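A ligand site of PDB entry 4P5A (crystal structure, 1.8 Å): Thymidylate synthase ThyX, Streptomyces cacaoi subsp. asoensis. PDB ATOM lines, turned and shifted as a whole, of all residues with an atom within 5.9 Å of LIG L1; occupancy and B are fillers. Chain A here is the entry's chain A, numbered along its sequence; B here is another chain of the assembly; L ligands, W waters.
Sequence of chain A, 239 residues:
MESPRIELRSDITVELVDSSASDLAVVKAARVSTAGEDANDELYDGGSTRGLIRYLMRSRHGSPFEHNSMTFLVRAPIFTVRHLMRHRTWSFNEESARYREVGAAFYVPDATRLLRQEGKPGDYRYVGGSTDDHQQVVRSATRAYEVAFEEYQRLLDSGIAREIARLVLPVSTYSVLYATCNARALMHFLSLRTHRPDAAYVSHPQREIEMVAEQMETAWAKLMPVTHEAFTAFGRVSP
Met 85 touches LIG L1. O of Glu 95 touches C1 of LIG L1, at 3.5 Å. Tyr 124 of chain B touches LIG L1. Hydrophobic or aromatic side chains that line LIG L1: Met 85, Ala 97, His 83 of chain B and Tyr 124 of chain B. Within 4 Å of LIG L1: Met 85, Glu 94, Glu 95, Ser 96, Ala 97, Arg 98, Arg 166, Arg 82 of chain B, His 83 of chain B, Arg 86 of chain B, Tyr 124 of chain B and Arg 193 of chain B.
The side-chain hydroxyl (OG) of Ser 96 lies within hydrogen-bond range of an oxygen (O2) of LIG L1 (2.5 Å). The guanidinium group (NH2) of Arg 166 lies within salt-bridge range of an oxygen (O3) of LIG L1, 2.7 Å away. OE1 of Glu 94 sits at hydrogen-bond distance from O6 of LIG L1 (2.7 Å). An oxygen (O3) of LIG L1 sits at hydrogen-bond distance from a ring nitrogen (NE2) of His 83 of chain B, at 2.7 Å. N of Arg 98 lies within hydrogen-bond range of O2 of LIG L1, 3.2 Å away. The guanidinium group (NH1) of Arg 98 lies within hydrogen-bond range of an oxygen (O9) of LIG L1 (2.8 Å). The guanidinium group (NH2) of Arg 193 of chain B is in hydrogen-bond range of an oxygen (O8) of LIG L1. The backbone NH (N) of Ala 97 sits at hydrogen-bond distance from an oxygen (O1) of LIG L1 (2.9 Å). The guanidinium group of Arg 86 of chain B lies within hydrogen-bond range of an oxygen (O6) of LIG L1, at 3.1 Å. O of Arg 82 of chain B is in hydrogen-bond range of O7 of LIG L1 (3.2 Å). The backbone NH (N) of Glu 94 sits at hydrogen-bond distance from an oxygen (O7) of LG2 L2, at 2.7 Å. The backbone carbonyl oxygen (O) of Glu 94 lies within hydrogen-bond range of a nitrogen (N7) of LG2 L2 (2.9 Å). An oxygen (O7) of LG2 L2 lies within hydrogen-bond range of the guanidinium group (NH2) of Arg 86 of chain B (2.8 Å).
The backbone NH (N) of Arg 98 sits at hydrogen-bond distance from the side-chain hydroxyl (OG) of Ser 96 (3.1 Å). N of Tyr 99 sits at hydrogen-bond distance from OG of Ser 96 (3.1 Å). The side-chain amide oxygen (OE1) of Gln 206 of chain B lies within hydrogen-bond range of the guanidinium group (NH2) of Arg 166, at 2.9 Å. OE2 of Glu 94 lies within salt-bridge range of NH1 of Arg 82 of chain B, at 3.0 Å. The backbone carbonyl oxygen (O) of His 83 of chain B sits at hydrogen-bond distance from the guanidinium group (NH2) of Arg 193 of chain B. The backbone carbonyl oxygen of His 204 of chain B sits at hydrogen-bond distance from the guanidinium group of Arg 98, 3.0 Å away.
A nitrogen (N7) of LG2 L2 lies close to an oxygen (O5) of LIG L1 (3.4 Å).
Water W3 bridges O1 of LIG L1 (2.4 Å) and NH1 of Arg 82 of chain B (3.2 Å). Water W2 lies within hydrogen-bond range of O9 of LIG L1 (2.7 Å), N of Gln 206 of chain B (2.8 Å), NH1 of Arg 193 of chain B (3.0 Å) and ND1 of His 83 of chain B (3.3 Å). Water W1 lies within hydrogen-bond range of an oxygen (O3) of LIG L1 (2.8 Å), the backbone carbonyl oxygen (O) of Phe 79 of chain B (2.9 Å) and a ring nitrogen (NE2) of His 83 of chain B (3.4 Å).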
ATOM      1  N   VAL A  81      -3.376 -18.510 -19.869  1.00  0.00           N
ATOM      2  CA  VAL A  81      -4.230 -17.321 -19.988  1.00  0.00           C
ATOM      3  C   VAL A  81      -5.250 -17.345 -18.897  1.00  0.00           C
ATOM      4  O   VAL A  81      -5.568 -16.262 -18.347  1.00  0.00           O
ATOM      5  CB  VAL A  81      -4.912 -17.300 -21.356  1.00  0.00           C
ATOM      6  CG1 VAL A  81      -5.916 -16.137 -21.437  1.00  0.00           C
ATOM      7  CG2 VAL A  81      -3.911 -17.139 -22.502  1.00  0.00           C
ATOM      8  N   MET A  85      -5.925 -14.257 -16.419  1.00  0.00           N
ATOM      9  CA  MET A  85      -7.220 -13.549 -16.382  1.00  0.00           C
ATOM     10  C   MET A  85      -7.938 -13.592 -15.062  1.00  0.00           C
ATOM     11  O   MET A  85      -9.063 -13.019 -14.942  1.00  0.00           O
ATOM     12  CB  MET A  85      -8.062 -14.051 -17.597  1.00  0.00           C
ATOM     13  CG  MET A  85      -7.331 -13.468 -18.856  1.00  0.00           C
ATOM     14  SD  MET A  85      -8.333 -13.948 -20.367  1.00  0.00           S
ATOM     15  CE  MET A  85      -9.639 -12.883 -20.250  1.00  0.00           C
ATOM     16  N   GLU A  94      -9.107 -10.733 -25.680  1.00  0.00           N
ATOM     17  CA  GLU A  94      -8.470 -11.935 -26.189  1.00  0.00           C
ATOM     18  C   GLU A  94      -9.061 -12.338 -27.535  1.00  0.00           C
ATOM     19  O   GLU A  94     -10.258 -12.124 -27.812  1.00  0.00           O
ATOM     20  CB  GLU A  94      -8.682 -13.067 -25.182  1.00  0.00           C
ATOM     21  CG  GLU A  94      -8.056 -14.414 -25.595  1.00  0.00           C
ATOM     22  CD  GLU A  94      -8.314 -15.515 -24.575  1.00  0.00           C
ATOM     23  OE1 GLU A  94      -8.927 -15.273 -23.484  1.00  0.00           O
ATOM     24  OE2 GLU A  94      -7.860 -16.676 -24.806  1.00  0.00           O
ATOM     25  N   GLU A  95      -8.275 -12.976 -28.394  1.00  0.00           N
ATOM     26  CA  GLU A  95      -8.861 -13.424 -29.651  1.00  0.00           C
ATOM     27  C   GLU A  95      -9.914 -14.585 -29.364  1.00  0.00           C
ATOM     28  O   GLU A  95      -9.803 -15.356 -28.416  1.00  0.00           O
ATOM     29  CB  GLU A  95      -7.754 -13.886 -30.647  1.00  0.00           C
ATOM     30  CG  GLU A  95      -7.222 -15.179 -30.322  1.00  0.00           C
ATOM     31  CD  GLU A  95      -6.219 -15.742 -31.437  1.00  0.00           C
ATOM     32  OE1 GLU A  95      -6.163 -15.186 -32.609  1.00  0.00           O
ATOM     33  OE2 GLU A  95      -5.491 -16.720 -31.066  1.00  0.00           O
ATOM     34  N   SER A  96     -10.963 -14.620 -30.154  1.00  0.00           N
ATOM     35  CA  SER A  96     -12.144 -15.522 -29.863  1.00  0.00           C
ATOM     36  C   SER A  96     -12.212 -16.740 -30.814  1.00  0.00           C
ATOM     37  O   SER A  96     -12.052 -16.555 -32.020  1.00  0.00           O
ATOM     38  CB  SER A  96     -13.357 -14.700 -30.128  1.00  0.00           C
ATOM     39  OG  SER A  96     -14.504 -15.507 -30.134  1.00  0.00           O
ATOM     40  N   ALA A  97     -12.348 -17.916 -30.263  1.00  0.00           N
ATOM     41  CA  ALA A  97     -12.576 -19.098 -31.088  1.00  0.00           C
ATOM     42  C   ALA A  97     -14.037 -19.211 -31.489  1.00  0.00           C
ATOM     43  O   ALA A  97     -14.367 -20.028 -32.346  1.00  0.00           O
ATOM     44  CB  ALA A  97     -12.070 -20.346 -30.319  1.00  0.00           C
ATOM     45  N   ARG A  98     -14.950 -18.429 -30.892  1.00  0.00           N
ATOM     46  CA  ARG A  98     -16.323 -18.352 -31.449  1.00  0.00           C
ATOM     47  C   ARG A  98     -16.284 -17.655 -32.803  1.00  0.00           C
ATOM     48  O   ARG A  98     -17.050 -17.959 -33.680  1.00  0.00           O
ATOM     49  CB  ARG A  98     -17.249 -17.526 -30.516  1.00  0.00           C
ATOM     50  CG  ARG A  98     -17.441 -18.220 -29.145  1.00  0.00           C
ATOM     51  CD  ARG A  98     -18.531 -17.430 -28.326  1.00  0.00           C
ATOM     52  NE  ARG A  98     -19.857 -17.606 -28.936  1.00  0.00           N
ATOM     53  CZ  ARG A  98     -20.846 -16.705 -28.890  1.00  0.00           C
ATOM     54  NH1 ARG A  98     -20.613 -15.518 -28.309  1.00  0.00           N
ATOM     55  NH2 ARG A  98     -22.036 -16.980 -29.498  1.00  0.00           N
ATOM     56  N   TYR A  99     -15.411 -16.679 -32.896  1.00  0.00           N
ATOM     57  CA  TYR A  99     -15.396 -15.710 -33.978  1.00  0.00           C
ATOM     58  C   TYR A  99     -14.494 -16.123 -35.131  1.00  0.00           C
ATOM     59  O   TYR A  99     -14.781 -15.785 -36.319  1.00  0.00           O
ATOM     60  CB  TYR A  99     -14.948 -14.335 -33.409  1.00  0.00           C
ATOM     61  CG  TYR A  99     -15.049 -13.208 -34.354  1.00  0.00           C
ATOM     62  CD1 TYR A  99     -16.189 -12.374 -34.360  1.00  0.00           C
ATOM     63  CD2 TYR A  99     -14.009 -12.928 -35.286  1.00  0.00           C
ATOM     64  CE1 TYR A  99     -16.304 -11.294 -35.301  1.00  0.00           C
ATOM     65  CE2 TYR A  99     -14.121 -11.867 -36.202  1.00  0.00           C
ATOM     66  CZ  TYR A  99     -15.269 -11.051 -36.194  1.00  0.00           C
ATOM     67  OH  TYR A  99     -15.390 -10.005 -37.104  1.00  0.00           O
ATOM     68  N   ARG A 166     -14.661 -26.136 -31.569  1.00  0.00           N
ATOM     69  CA  ARG A 166     -13.495 -25.929 -30.730  1.00  0.00           C
ATOM     70  C   ARG A 166     -13.575 -26.692 -29.420  1.00  0.00           C
ATOM     71  O   ARG A 166     -12.582 -26.684 -28.638  1.00  0.00           O
ATOM     72  CB  ARG A 166     -13.247 -24.391 -30.445  1.00  0.00           C
ATOM     73  CG  ARG A 166     -14.379 -23.645 -29.727  1.00  0.00           C
ATOM     74  CD  ARG A 166     -14.676 -24.030 -28.303  1.00  0.00           C
ATOM     75  NE  ARG A 166     -15.639 -23.022 -27.813  1.00  0.00           N
ATOM     76  CZ  ARG A 166     -15.280 -21.783 -27.376  1.00  0.00           C
ATOM     77  NH1 ARG A 166     -14.009 -21.440 -27.205  1.00  0.00           N
ATOM     78  NH2 ARG A 166     -16.240 -20.900 -27.125  1.00  0.00           N
ATOM     79  N   PHE B  79     -14.685 -24.199 -21.388  1.00  0.00           N
ATOM     80  CA  PHE B  79     -14.942 -23.057 -22.236  1.00  0.00           C
ATOM     81  C   PHE B  79     -16.054 -22.133 -21.752  1.00  0.00           C
ATOM     82  O   PHE B  79     -16.054 -20.958 -22.095  1.00  0.00           O
ATOM     83  CB  PHE B  79     -15.154 -23.408 -23.715  1.00  0.00           C
ATOM     84  CG  PHE B  79     -16.452 -24.112 -23.998  1.00  0.00           C
ATOM     85  CD1 PHE B  79     -16.590 -25.501 -23.803  1.00  0.00           C
ATOM     86  CD2 PHE B  79     -17.563 -23.348 -24.383  1.00  0.00           C
ATOM     87  CE1 PHE B  79     -17.870 -26.124 -24.036  1.00  0.00           C
ATOM     88  CE2 PHE B  79     -18.817 -23.950 -24.576  1.00  0.00           C
ATOM     89  CZ  PHE B  79     -18.969 -25.319 -24.353  1.00  0.00           C
ATOM     90  N   ARG B  82     -14.833 -20.105 -18.618  1.00  0.00           N
ATOM     91  CA  ARG B  82     -14.114 -18.920 -19.099  1.00  0.00           C
ATOM     92  C   ARG B  82     -15.067 -17.740 -19.292  1.00  0.00           C
ATOM     93  O   ARG B  82     -14.626 -16.638 -18.920  1.00  0.00           O
ATOM     94  CB  ARG B  82     -13.300 -19.124 -20.385  1.00  0.00           C
ATOM     95  CG  ARG B  82     -12.297 -20.301 -20.181  1.00  0.00           C
ATOM     96  CD  ARG B  82     -10.889 -19.824 -20.711  1.00  0.00           C
ATOM     97  NE  ARG B  82     -10.775 -19.576 -22.074  1.00  0.00           N
ATOM     98  CZ  ARG B  82      -9.932 -18.682 -22.623  1.00  0.00           C
ATOM     99  NH1 ARG B  82      -9.846 -18.677 -23.894  1.00  0.00           N
ATOM    100  NH2 ARG B  82      -9.203 -17.804 -21.938  1.00  0.00           N
ATOM    101  N   HIS B  83     -16.209 -17.927 -19.944  1.00  0.00           N
ATOM    102  CA  HIS B  83     -17.148 -16.844 -20.131  1.00  0.00           C
ATOM    103  C   HIS B  83     -17.610 -16.286 -18.757  1.00  0.00           C
ATOM    104  O   HIS B  83     -17.615 -15.071 -18.606  1.00  0.00           O
ATOM    105  CB  HIS B  83     -18.352 -17.276 -20.988  1.00  0.00           C
ATOM    106  CG  HIS B  83     -17.917 -17.788 -22.323  1.00  0.00           C
ATOM    107  ND1 HIS B  83     -18.773 -18.458 -23.183  1.00  0.00           N
ATOM    108  CD2 HIS B  83     -16.730 -17.660 -22.964  1.00  0.00           C
ATOM    109  CE1 HIS B  83     -18.114 -18.737 -24.300  1.00  0.00           C
ATOM    110  NE2 HIS B  83     -16.897 -18.217 -24.221  1.00  0.00           N
ATOM    111  N   LEU B  84     -17.997 -17.174 -17.868  1.00  0.00           N
ATOM    112  CA  LEU B  84     -18.489 -16.758 -16.503  1.00  0.00           C
ATOM    113  C   LEU B  84     -17.386 -15.947 -15.833  1.00  0.00           C
ATOM    114  O   LEU B  84     -17.693 -14.877 -15.245  1.00  0.00           O
ATOM    115  CB  LEU B  84     -18.773 -18.004 -15.654  1.00  0.00           C
ATOM    116  CG  LEU B  84     -19.143 -17.678 -14.198  1.00  0.00           C
ATOM    117  CD1 LEU B  84     -20.352 -16.719 -14.135  1.00  0.00           C
ATOM    118  CD2 LEU B  84     -19.581 -19.012 -13.580  1.00  0.00           C
ATOM    119  N   ARG B  86     -15.034 -14.018 -16.837  1.00  0.00           N
ATOM    120  CA  ARG B  86     -14.741 -12.686 -17.281  1.00  0.00           C
ATOM    121  C   ARG B  86     -15.456 -11.551 -16.454  1.00  0.00           C
ATOM    122  O   ARG B  86     -15.058 -10.368 -16.541  1.00  0.00           O
ATOM    123  CB  ARG B  86     -15.126 -12.464 -18.745  1.00  0.00           C
ATOM    124  CG  ARG B  86     -14.298 -13.385 -19.667  1.00  0.00           C
ATOM    125  CD  ARG B  86     -12.749 -13.152 -19.492  1.00  0.00           C
ATOM    126  NE  ARG B  86     -12.394 -11.707 -19.779  1.00  0.00           N
ATOM    127  CZ  ARG B  86     -12.145 -11.220 -21.005  1.00  0.00           C
ATOM    128  NH1 ARG B  86     -11.893  -9.929 -21.153  1.00  0.00           N
ATOM    129  NH2 ARG B  86     -12.214 -11.988 -22.119  1.00  0.00           N
ATOM    130  N   TYR B 124     -23.327 -13.619 -34.805  1.00  0.00           N
ATOM    131  CA  TYR B 124     -23.536 -14.761 -33.887  1.00  0.00           C
ATOM    132  C   TYR B 124     -24.950 -15.440 -34.114  1.00  0.00           C
ATOM    133  O   TYR B 124     -25.664 -15.812 -33.151  1.00  0.00           O
ATOM    134  CB  TYR B 124     -23.187 -14.381 -32.403  1.00  0.00           C
ATOM    135  CG  TYR B 124     -21.691 -14.073 -32.134  1.00  0.00           C
ATOM    136  CD1 TYR B 124     -20.737 -15.081 -32.197  1.00  0.00           C
ATOM    137  CD2 TYR B 124     -21.236 -12.773 -31.849  1.00  0.00           C
ATOM    138  CE1 TYR B 124     -19.354 -14.818 -31.995  1.00  0.00           C
ATOM    139  CE2 TYR B 124     -19.835 -12.503 -31.602  1.00  0.00           C
ATOM    140  CZ  TYR B 124     -18.915 -13.554 -31.679  1.00  0.00           C
ATOM    141  OH  TYR B 124     -17.549 -13.384 -31.468  1.00  0.00           O
ATOM    142  N   ARG B 193     -25.380 -12.174 -20.825  1.00  0.00           N
ATOM    143  CA  ARG B 193     -25.258 -13.638 -20.987  1.00  0.00           C
ATOM    144  C   ARG B 193     -26.644 -14.303 -21.210  1.00  0.00           C
ATOM    145  O   ARG B 193     -26.743 -15.528 -21.116  1.00  0.00           O
ATOM    146  CB  ARG B 193     -24.570 -14.314 -19.798  1.00  0.00           C
ATOM    147  CG  ARG B 193     -23.176 -13.773 -19.589  1.00  0.00           C
ATOM    148  CD  ARG B 193     -22.242 -13.913 -20.823  1.00  0.00           C
ATOM    149  NE  ARG B 193     -20.816 -13.548 -20.446  1.00  0.00           N
ATOM    150  CZ  ARG B 193     -19.806 -13.705 -21.315  1.00  0.00           C
ATOM    151  NH1 ARG B 193     -20.061 -14.207 -22.581  1.00  0.00           N
ATOM    152  NH2 ARG B 193     -18.560 -13.428 -20.922  1.00  0.00           N
ATOM    153  N   HIS B 204     -25.480 -11.740 -27.744  1.00  0.00           N
ATOM    154  CA  HIS B 204     -25.422 -13.031 -28.449  1.00  0.00           C
ATOM    155  C   HIS B 204     -24.419 -13.933 -27.738  1.00  0.00           C
ATOM    156  O   HIS B 204     -23.409 -14.341 -28.316  1.00  0.00           O
ATOM    157  CB  HIS B 204     -24.926 -12.760 -29.890  1.00  0.00           C
ATOM    158  CG  HIS B 204     -25.941 -12.047 -30.703  1.00  0.00           C
ATOM    159  ND1 HIS B 204     -27.120 -12.652 -31.060  1.00  0.00           N
ATOM    160  CD2 HIS B 204     -26.038 -10.748 -31.072  1.00  0.00           C
ATOM    161  CE1 HIS B 204     -27.891 -11.765 -31.666  1.00  0.00           C
ATOM    162  NE2 HIS B 204     -27.257 -10.611 -31.697  1.00  0.00           N
ATOM    163  N   PRO B 205     -24.670 -14.269 -26.456  1.00  0.00           N
ATOM    164  CA  PRO B 205     -23.746 -15.175 -25.797  1.00  0.00           C
ATOM    165  C   PRO B 205     -23.866 -16.586 -26.369  1.00  0.00           C
ATOM    166  O   PRO B 205     -24.947 -17.001 -26.904  1.00  0.00           O
ATOM    167  CB  PRO B 205     -24.334 -15.232 -24.359  1.00  0.00           C
ATOM    168  CG  PRO B 205     -25.842 -15.042 -24.550  1.00  0.00           C
ATOM    169  CD  PRO B 205     -25.872 -13.964 -25.654  1.00  0.00           C
ATOM    170  N   GLN B 206     -22.851 -17.351 -26.163  1.00  0.00           N
ATOM    171  CA  GLN B 206     -22.886 -18.763 -26.439  1.00  0.00           C
ATOM    172  C   GLN B 206     -23.980 -19.483 -25.679  1.00  0.00           C
ATOM    173  O   GLN B 206     -24.228 -19.194 -24.507  1.00  0.00           O
ATOM    174  CB  GLN B 206     -21.497 -19.397 -26.175  1.00  0.00           C
ATOM    175  CG  GLN B 206     -21.455 -20.907 -26.533  1.00  0.00           C
ATOM    176  CD  GLN B 206     -20.115 -21.442 -27.041  1.00  0.00           C
ATOM    177  OE1 GLN B 206     -19.184 -20.727 -27.190  1.00  0.00           O
ATOM    178  NE2 GLN B 206     -20.085 -22.788 -27.465  1.00  0.00           N
HETATM  179  P1  LIG L   1     -14.011 -17.788 -26.962  1.00  0.00           P
HETATM  180  O1  LIG L   1     -12.793 -18.544 -27.419  1.00  0.00           O
HETATM  181  O2  LIG L   1     -14.689 -16.925 -28.039  1.00  0.00           O
HETATM  182  O3  LIG L   1     -15.050 -18.690 -26.185  1.00  0.00           O
HETATM  183  O4  LIG L   1     -13.472 -16.706 -25.863  1.00  0.00           O
HETATM  184  C1  LIG L   1     -12.293 -16.087 -26.088  1.00  0.00           C
HETATM  185  C2  LIG L   1     -12.043 -15.041 -24.866  1.00  0.00           C
HETATM  186  O5  LIG L   1     -13.125 -14.041 -24.920  1.00  0.00           O
HETATM  187  C3  LIG L   1     -12.199 -15.705 -23.507  1.00  0.00           C
HETATM  188  O6  LIG L   1     -11.458 -14.958 -22.496  1.00  0.00           O
HETATM  189  C4  LIG L   1     -13.679 -15.502 -23.234  1.00  0.00           C
HETATM  190  O7  LIG L   1     -13.938 -15.523 -21.815  1.00  0.00           O
HETATM  191  C5  LIG L   1     -14.076 -14.184 -23.886  1.00  0.00           C
HETATM  192  N1  LIG L   1     -15.393 -14.204 -24.565  1.00  0.00           N
HETATM  193  C6  LIG L   1     -16.517 -14.370 -23.769  1.00  0.00           C
HETATM  194  O8  LIG L   1     -16.344 -14.346 -22.528  1.00  0.00           O
HETATM  195  N2  LIG L   1     -17.764 -14.551 -24.276  1.00  0.00           N
HETATM  196  C7  LIG L   1     -17.937 -14.555 -25.659  1.00  0.00           C
HETATM  197  O9  LIG L   1     -19.038 -14.698 -26.124  1.00  0.00           O
HETATM  198  C8  LIG L   1     -16.772 -14.390 -26.436  1.00  0.00           C
HETATM  199  C9  LIG L   1     -15.508 -14.252 -25.977  1.00  0.00           C
HETATM  200 BR1  LIG L   1     -17.003 -14.192 -28.350  1.00  0.00          BR
HETATM  201  P1  LG2 L   2     -17.449  -6.940 -15.514  1.00  0.00           P
HETATM  202  O1  LG2 L   2     -18.334  -7.608 -14.549  1.00  0.00           O
HETATM  203  O2  LG2 L   2     -16.071  -7.299 -15.670  1.00  0.00           O
HETATM  204  O3  LG2 L   2     -17.562  -5.408 -15.274  1.00  0.00           O
HETATM  205  C1  LG2 L   2     -18.891  -4.760 -15.119  1.00  0.00           C
HETATM  206  C2  LG2 L   2     -18.784  -3.284 -15.387  1.00  0.00           C
HETATM  207  O4  LG2 L   2     -17.823  -2.717 -14.472  1.00  0.00           O
HETATM  208  C3  LG2 L   2     -18.221  -2.995 -16.738  1.00  0.00           C
HETATM  209  O5  LG2 L   2     -19.259  -3.007 -17.755  1.00  0.00           O
HETATM  210  C4  LG2 L   2     -17.629  -1.578 -16.595  1.00  0.00           C
HETATM  211  O6  LG2 L   2     -18.774  -0.649 -16.513  1.00  0.00           O
HETATM  212  C5  LG2 L   2     -17.041  -1.655 -15.149  1.00  0.00           C
HETATM  213  N1  LG2 L   2     -15.614  -2.033 -15.090  1.00  0.00           N
HETATM  214  C6  LG2 L   2     -15.120  -3.051 -14.362  1.00  0.00           C
HETATM  215  N2  LG2 L   2     -13.791  -3.078 -14.447  1.00  0.00           N
HETATM  216  C7  LG2 L   2     -13.417  -1.978 -15.215  1.00  0.00           C
HETATM  217  C8  LG2 L   2     -12.203  -1.423 -15.688  1.00  0.00           C
HETATM  218  N3  LG2 L   2     -10.985  -1.933 -15.362  1.00  0.00           N
HETATM  219  N4  LG2 L   2     -12.286  -0.305 -16.488  1.00  0.00           N
HETATM  220  C9  LG2 L   2     -13.466   0.287 -16.785  1.00  0.00           C
HETATM  221  N5  LG2 L   2     -14.656  -0.215 -16.357  1.00  0.00           N
HETATM  222  C10 LG2 L   2     -14.629  -1.358 -15.629  1.00  0.00           C
HETATM  223  N6  LG2 L   2     -13.895 -10.899 -24.606  1.00  0.00           N
HETATM  224  C11 LG2 L   2     -12.689 -10.969 -25.257  1.00  0.00           C
HETATM  225  O7  LG2 L   2     -11.612 -11.022 -24.682  1.00  0.00           O
HETATM  226  N7  LG2 L   2     -12.687 -11.136 -26.621  1.00  0.00           N
HETATM  227  C12 LG2 L   2     -13.881 -11.233 -27.333  1.00  0.00           C
HETATM  228  O8  LG2 L   2     -13.772 -11.318 -28.585  1.00  0.00           O
HETATM  229  C13 LG2 L   2     -15.112 -11.132 -26.659  1.00  0.00           C
HETATM  230  N8  LG2 L   2     -16.358 -11.081 -27.325  1.00  0.00           N
HETATM  231  C14 LG2 L   2     -17.553 -11.174 -26.553  1.00  0.00           C
HETATM  232  C15 LG2 L   2     -18.834 -11.397 -27.106  1.00  0.00           C
HETATM  233  C16 LG2 L   2     -20.004 -11.454 -26.332  1.00  0.00           C
HETATM  234  C17 LG2 L   2     -21.306 -11.704 -27.108  1.00  0.00           C
HETATM  235  C18 LG2 L   2     -19.985 -11.368 -24.914  1.00  0.00           C
HETATM  236  C19 LG2 L   2     -21.267 -11.365 -24.029  1.00  0.00           C
HETATM  237  C20 LG2 L   2     -18.713 -11.160 -24.323  1.00  0.00           C
HETATM  238  C21 LG2 L   2     -17.520 -11.121 -25.126  1.00  0.00           C
HETATM  239  N9  LG2 L   2     -16.249 -10.908 -24.523  1.00  0.00           N
HETATM  240  C22 LG2 L   2     -15.083 -10.970 -25.298  1.00  0.00           C
HETATM  241  C23 LG2 L   2     -16.116 -10.853 -23.034  1.00  0.00           C
HETATM  242  C24 LG2 L   2     -16.434  -9.310 -22.762  1.00  0.00           C
HETATM  243  O9  LG2 L   2     -15.407  -8.427 -23.322  1.00  0.00           O
HETATM  244  C25 LG2 L   2     -16.366  -9.019 -21.238  1.00  0.00           C
HETATM  245  O10 LG2 L   2     -15.143  -9.462 -20.630  1.00  0.00           O
HETATM  246  C26 LG2 L   2     -17.580  -9.758 -20.448  1.00  0.00           C
HETATM  247  O11 LG2 L   2     -18.729  -9.664 -21.219  1.00  0.00           O
HETATM  248  C27 LG2 L   2     -17.747  -9.071 -19.068  1.00  0.00           C
HETATM  249  O12 LG2 L   2     -18.409  -7.807 -19.282  1.00  0.00           O
HETATM  250  P2  LG2 L   2     -17.929  -6.560 -18.388  1.00  0.00           P
HETATM  251  O13 LG2 L   2     -16.477  -6.234 -18.528  1.00  0.00           O
HETATM  252  O14 LG2 L   2     -18.854  -5.478 -18.768  1.00  0.00           O
HETATM  253  O15 LG2 L   2     -18.184  -7.040 -16.893  1.00  0.00           O
HETATM  254  O   HOH W   1     -14.006 -19.966 -23.917  1.00  0.00           O
HETATM  255  O   HOH W   2     -20.722 -16.281 -24.651  1.00  0.00           O
HETATM  256  O   HOH W   3     -10.638 -19.552 -26.913  1.00  0.00           O
